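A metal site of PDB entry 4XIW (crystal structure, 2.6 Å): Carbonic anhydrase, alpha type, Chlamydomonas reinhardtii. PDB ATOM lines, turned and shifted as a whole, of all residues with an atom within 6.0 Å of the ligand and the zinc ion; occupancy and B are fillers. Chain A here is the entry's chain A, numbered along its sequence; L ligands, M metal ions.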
ATOM      1  N   LEU A  86     -14.049 -23.605  11.822  1.00  0.00           N
ATOM      2  CA  LEU A  86     -13.023 -24.324  12.527  1.00  0.00           C
ATOM      3  C   LEU A  86     -13.456 -24.517  13.982  1.00  0.00           C
ATOM      4  O   LEU A  86     -13.510 -25.642  14.456  1.00  0.00           O
ATOM      5  CB  LEU A  86     -11.720 -23.546  12.458  1.00  0.00           C
ATOM      6  CG  LEU A  86     -11.276 -23.263  11.050  1.00  0.00           C
ATOM      7  CD1 LEU A  86     -10.085 -22.341  11.025  1.00  0.00           C
ATOM      8  CD2 LEU A  86     -10.927 -24.580  10.321  1.00  0.00           C
ATOM      9  N   GLN A  87     -13.755 -23.399  14.663  1.00  0.00           N
ATOM     10  CA  GLN A  87     -14.081 -23.379  16.115  1.00  0.00           C
ATOM     11  C   GLN A  87     -14.874 -22.151  16.485  1.00  0.00           C
ATOM     12  O   GLN A  87     -14.815 -21.135  15.777  1.00  0.00           O
ATOM     13  CB  GLN A  87     -12.840 -23.301  16.951  1.00  0.00           C
ATOM     14  CG  GLN A  87     -11.903 -22.151  16.473  1.00  0.00           C
ATOM     15  CD  GLN A  87     -11.623 -21.037  17.484  1.00  0.00           C
ATOM     16  OE1 GLN A  87     -12.423 -20.730  18.391  1.00  0.00           O
ATOM     17  NE2 GLN A  87     -10.459 -20.399  17.302  1.00  0.00           N
ATOM     18  N   HIS A  89     -15.505 -19.571  20.182  1.00  0.00           N
ATOM     19  CA  HIS A  89     -15.204 -19.218  21.605  1.00  0.00           C
ATOM     20  C   HIS A  89     -15.855 -17.875  21.973  1.00  0.00           C
ATOM     21  O   HIS A  89     -16.552 -17.266  21.149  1.00  0.00           O
ATOM     22  CB  HIS A  89     -13.692 -19.139  21.855  1.00  0.00           C
ATOM     23  CG  HIS A  89     -13.016 -18.130  20.980  1.00  0.00           C
ATOM     24  ND1 HIS A  89     -12.551 -18.437  19.723  1.00  0.00           N
ATOM     25  CD2 HIS A  89     -12.795 -16.807  21.152  1.00  0.00           C
ATOM     26  CE1 HIS A  89     -12.034 -17.353  19.174  1.00  0.00           C
ATOM     27  NE2 HIS A  89     -12.167 -16.344  20.019  1.00  0.00           N
ATOM     28  N   PHE A  90     -15.594 -17.380  23.182  1.00  0.00           N
ATOM     29  CA  PHE A  90     -16.230 -16.143  23.630  1.00  0.00           C
ATOM     30  C   PHE A  90     -15.301 -15.103  24.258  1.00  0.00           C
ATOM     31  O   PHE A  90     -14.181 -15.387  24.659  1.00  0.00           O
ATOM     32  CB  PHE A  90     -17.368 -16.483  24.586  1.00  0.00           C
ATOM     33  CG  PHE A  90     -18.354 -17.511  24.048  1.00  0.00           C
ATOM     34  CD1 PHE A  90     -18.103 -18.867  24.169  1.00  0.00           C
ATOM     35  CD2 PHE A  90     -19.552 -17.099  23.440  1.00  0.00           C
ATOM     36  CE1 PHE A  90     -19.043 -19.817  23.695  1.00  0.00           C
ATOM     37  CE2 PHE A  90     -20.471 -18.005  22.997  1.00  0.00           C
ATOM     38  CZ  PHE A  90     -20.216 -19.370  23.121  1.00  0.00           C
ATOM     39  N   HIS A  91     -15.799 -13.863  24.292  1.00  0.00           N
ATOM     40  CA  HIS A  91     -15.161 -12.783  25.017  1.00  0.00           C
ATOM     41  C   HIS A  91     -16.204 -11.975  25.795  1.00  0.00           C
ATOM     42  O   HIS A  91     -17.329 -11.758  25.302  1.00  0.00           O
ATOM     43  CB  HIS A  91     -14.441 -11.854  24.075  1.00  0.00           C
ATOM     44  CG  HIS A  91     -13.405 -12.527  23.259  1.00  0.00           C
ATOM     45  ND1 HIS A  91     -12.068 -12.453  23.549  1.00  0.00           N
ATOM     46  CD2 HIS A  91     -13.515 -13.260  22.129  1.00  0.00           C
ATOM     47  CE1 HIS A  91     -11.379 -13.126  22.647  1.00  0.00           C
ATOM     48  NE2 HIS A  91     -12.235 -13.630  21.776  1.00  0.00           N
ATOM     49  N   GLU A  95     -15.762  -7.500  22.262  1.00  0.00           N
ATOM     50  CA  GLU A  95     -14.440  -6.919  21.949  1.00  0.00           C
ATOM     51  C   GLU A  95     -14.662  -5.821  20.951  1.00  0.00           C
ATOM     52  O   GLU A  95     -14.048  -4.762  21.000  1.00  0.00           O
ATOM     53  CB  GLU A  95     -13.471  -7.957  21.399  1.00  0.00           C
ATOM     54  CG  GLU A  95     -13.157  -9.104  22.359  1.00  0.00           C
ATOM     55  CD  GLU A  95     -11.824  -9.749  22.039  1.00  0.00           C
ATOM     56  OE1 GLU A  95     -11.731 -10.502  21.043  1.00  0.00           O
ATOM     57  OE2 GLU A  95     -10.851  -9.468  22.765  1.00  0.00           O
ATOM     58  N   HIS A 108     -17.274 -15.526  18.804  1.00  0.00           N
ATOM     59  CA  HIS A 108     -16.396 -15.523  17.665  1.00  0.00           C
ATOM     60  C   HIS A 108     -16.377 -16.880  16.989  1.00  0.00           C
ATOM     61  O   HIS A 108     -15.893 -17.853  17.586  1.00  0.00           O
ATOM     62  CB  HIS A 108     -15.002 -15.237  18.126  1.00  0.00           C
ATOM     63  CG  HIS A 108     -14.741 -13.790  18.332  1.00  0.00           C
ATOM     64  ND1 HIS A 108     -13.543 -13.321  18.831  1.00  0.00           N
ATOM     65  CD2 HIS A 108     -15.512 -12.694  18.121  1.00  0.00           C
ATOM     66  CE1 HIS A 108     -13.586 -12.004  18.919  1.00  0.00           C
ATOM     67  NE2 HIS A 108     -14.771 -11.597  18.492  1.00  0.00           N
ATOM     68  N   VAL A 110     -14.813 -18.917  14.136  1.00  0.00           N
ATOM     69  CA  VAL A 110     -13.630 -18.744  13.312  1.00  0.00           C
ATOM     70  C   VAL A 110     -13.677 -19.711  12.112  1.00  0.00           C
ATOM     71  O   VAL A 110     -14.051 -20.858  12.253  1.00  0.00           O
ATOM     72  CB  VAL A 110     -12.367 -18.953  14.126  1.00  0.00           C
ATOM     73  CG1 VAL A 110     -11.175 -18.533  13.333  1.00  0.00           C
ATOM     74  CG2 VAL A 110     -12.427 -18.164  15.436  1.00  0.00           C
ATOM     75  N   LEU A 119      -7.850 -16.754   7.215  1.00  0.00           N
ATOM     76  CA  LEU A 119      -8.870 -16.891   8.261  1.00  0.00           C
ATOM     77  C   LEU A 119      -9.974 -15.836   8.173  1.00  0.00           C
ATOM     78  O   LEU A 119      -9.711 -14.669   7.871  1.00  0.00           O
ATOM     79  CB  LEU A 119      -8.211 -16.789   9.621  1.00  0.00           C
ATOM     80  CG  LEU A 119      -7.394 -17.987  10.093  1.00  0.00           C
ATOM     81  CD1 LEU A 119      -6.631 -17.555  11.351  1.00  0.00           C
ATOM     82  CD2 LEU A 119      -8.287 -19.183  10.398  1.00  0.00           C
ATOM     83  N   VAL A 121     -13.363 -14.365  10.642  1.00  0.00           N
ATOM     84  CA  VAL A 121     -14.064 -14.503  11.919  1.00  0.00           C
ATOM     85  C   VAL A 121     -15.408 -13.786  11.903  1.00  0.00           C
ATOM     86  O   VAL A 121     -15.532 -12.632  11.465  1.00  0.00           O
ATOM     87  CB  VAL A 121     -13.241 -13.976  13.129  1.00  0.00           C
ATOM     88  CG1 VAL A 121     -13.867 -14.463  14.431  1.00  0.00           C
ATOM     89  CG2 VAL A 121     -11.808 -14.454  13.067  1.00  0.00           C
ATOM     90  N   SER A 181      -7.339  -8.385  12.492  1.00  0.00           N
ATOM     91  CA  SER A 181      -6.384  -9.350  13.045  1.00  0.00           C
ATOM     92  C   SER A 181      -6.991 -10.331  14.048  1.00  0.00           C
ATOM     93  O   SER A 181      -8.161 -10.212  14.428  1.00  0.00           O
ATOM     94  CB  SER A 181      -5.230  -8.588  13.728  1.00  0.00           C
ATOM     95  OG  SER A 181      -5.673  -7.867  14.869  1.00  0.00           O
ATOM     96  N   LEU A 182      -6.198 -11.310  14.482  1.00  0.00           N
ATOM     97  CA  LEU A 182      -6.560 -12.072  15.645  1.00  0.00           C
ATOM     98  C   LEU A 182      -6.556 -11.052  16.787  1.00  0.00           C
ATOM     99  O   LEU A 182      -5.871 -10.017  16.691  1.00  0.00           O
ATOM    100  CB  LEU A 182      -5.573 -13.209  15.872  1.00  0.00           C
ATOM    101  CG  LEU A 182      -5.478 -14.148  14.654  1.00  0.00           C
ATOM    102  CD1 LEU A 182      -4.426 -15.198  14.835  1.00  0.00           C
ATOM    103  CD2 LEU A 182      -6.789 -14.827  14.465  1.00  0.00           C
ATOM    104  N   THR A 183      -7.338 -11.302  17.842  1.00  0.00           N
ATOM    105  CA  THR A 183      -7.416 -10.355  18.949  1.00  0.00           C
ATOM    106  C   THR A 183      -6.521 -10.802  20.121  1.00  0.00           C
ATOM    107  O   THR A 183      -6.524 -10.177  21.196  1.00  0.00           O
ATOM    108  CB  THR A 183      -8.873 -10.189  19.444  1.00  0.00           C
ATOM    109  OG1 THR A 183      -9.387 -11.444  19.888  1.00  0.00           O
ATOM    110  CG2 THR A 183      -9.765  -9.629  18.367  1.00  0.00           C
ATOM    111  N   THR A 184      -5.768 -11.861  19.900  1.00  0.00           N
ATOM    112  CA  THR A 184      -4.863 -12.399  20.918  1.00  0.00           C
ATOM    113  C   THR A 184      -3.556 -12.677  20.198  1.00  0.00           C
ATOM    114  O   THR A 184      -3.566 -12.876  18.989  1.00  0.00           O
ATOM    115  CB  THR A 184      -5.406 -13.710  21.487  1.00  0.00           C
ATOM    116  OG1 THR A 184      -5.416 -14.711  20.452  1.00  0.00           O
ATOM    117  CG2 THR A 184      -6.788 -13.515  21.993  1.00  0.00           C
ATOM    118  N   PRO A 185      -2.426 -12.655  20.921  1.00  0.00           N
ATOM    119  CA  PRO A 185      -1.127 -12.951  20.302  1.00  0.00           C
ATOM    120  C   PRO A 185      -1.183 -14.238  19.456  1.00  0.00           C
ATOM    121  O   PRO A 185      -1.848 -15.177  19.887  1.00  0.00           O
ATOM    122  CB  PRO A 185      -0.221 -13.127  21.505  1.00  0.00           C
ATOM    123  CG  PRO A 185      -0.798 -12.283  22.513  1.00  0.00           C
ATOM    124  CD  PRO A 185      -2.283 -12.347  22.339  1.00  0.00           C
ATOM    125  N   TRP A 193     -12.933  -9.935   8.993  1.00  0.00           N
ATOM    126  CA  TRP A 193     -13.854  -9.822  10.124  1.00  0.00           C
ATOM    127  C   TRP A 193     -15.231  -9.503   9.609  1.00  0.00           C
ATOM    128  O   TRP A 193     -15.410  -8.527   8.848  1.00  0.00           O
ATOM    129  CB  TRP A 193     -13.382  -8.730  11.138  1.00  0.00           C
ATOM    130  CG  TRP A 193     -12.478  -9.261  12.107  1.00  0.00           C
ATOM    131  CD1 TRP A 193     -11.111  -9.217  12.074  1.00  0.00           C
ATOM    132  CD2 TRP A 193     -12.828  -9.996  13.266  1.00  0.00           C
ATOM    133  NE1 TRP A 193     -10.605  -9.869  13.163  1.00  0.00           N
ATOM    134  CE2 TRP A 193     -11.642 -10.369  13.905  1.00  0.00           C
ATOM    135  CE3 TRP A 193     -14.054 -10.380  13.825  1.00  0.00           C
ATOM    136  CZ2 TRP A 193     -11.636 -11.106  15.091  1.00  0.00           C
ATOM    137  CZ3 TRP A 193     -14.039 -11.115  15.008  1.00  0.00           C
ATOM    138  CH2 TRP A 193     -12.838 -11.465  15.620  1.00  0.00           C
HETATM  139  C1  LIG L   1      -8.787 -15.461  17.890  1.00  0.00           C
HETATM  140  C2  LIG L   1      -6.997 -17.279  17.233  1.00  0.00           C
HETATM  141  C3  LIG L   1      -6.551 -19.134  15.772  1.00  0.00           C
HETATM  142  C4  LIG L   1      -5.594 -20.221  15.338  1.00  0.00           C
HETATM  143  N1  LIG L   1     -10.468 -13.962  19.333  1.00  0.00           N
HETATM  144  N2  LIG L   1      -6.781 -16.377  18.189  1.00  0.00           N
HETATM  145  N3  LIG L   1      -7.633 -15.494  18.518  1.00  0.00           N
HETATM  146  N4  LIG L   1      -6.177 -18.302  16.773  1.00  0.00           N
HETATM  147  O1  LIG L   1      -9.314 -13.078  17.272  1.00  0.00           O
HETATM  148  O2  LIG L   1     -11.066 -14.859  17.107  1.00  0.00           O
HETATM  149  O3  LIG L   1      -7.633 -19.058  15.241  1.00  0.00           O
HETATM  150  S1  LIG L   1      -9.990 -14.220  17.777  1.00  0.00           S
HETATM  151  S2  LIG L   1      -8.586 -16.816  16.767  1.00  0.00           S
HETATM  152 ZN    ZN M   1     -12.100 -14.317  19.877  1.00  0.00          ZN
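The side-chain hydroxyl (OG1) of Thr 183 lies within hydrogen-bond range of an oxygen (O1) of the ligand (3.1 Å). The backbone NH (N) of Thr 183 is in hydrogen-bond range of an oxygen (O1) of the ligand. The side-chain hydroxyl (OG1) of Thr 184 is in hydrogen-bond range of a nitrogen (N3) of the ligand, at 3.0 Å.
The backbone carbonyl oxygen of Gln 87 lies within hydrogen-bond range of the backbone NH of Val 110 (2.8 Å). OG1 of Thr 183 sits at hydrogen-bond distance from OE1 of Glu 95, 2.8 Å away. A ring nitrogen (ND1) of His 91 sits close to the side-chain carboxylate (OE1) of Glu 95, 3.2 Å away. A ring nitrogen (ND1) of His 89 is in hydrogen-bond range of the side-chain amide oxygen of Gln 87, at 2.7 Å. The backbone carbonyl oxygen (O) of Val 110 sits at hydrogen-bond distance from the backbone NH (N) of Leu 86, 2.8 Å away. The indole nitrogen (NE1) of Trp 193 lies within hydrogen-bond range of the backbone carbonyl oxygen (O) of Ser 181.
Residues that only touch the ligand: Gln 87 (3.7 Å), Val 110 (3.9 Å), Val 121 (3.9 Å), Leu 182 (3.4 Å) and Trp 193 (3.7 Å). Hydrophobic or aromatic side chains that line the ligand: His 89, His 91, His 108, Val 110, Val 121, Leu 182 and Trp 193. Ten residues have an atom within 4 Å of the ligand: Gln 87, His 89, His 91, His 108, Val 110, Val 121, Leu 182, Thr 183, Thr 184 and Trp 193.
Residues that only touch the zinc ion: Thr 183. The nearest printed residue that does not touch the zinc ion is Glu 95 (4.01 Å).
The zinc ion is bound by N1 of the ligand (1.8 Å), NE2 of His 91 (2.0 Å), NE2 of His 89 (2.0 Å) and ND1 of His 108 (2.0 Å).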
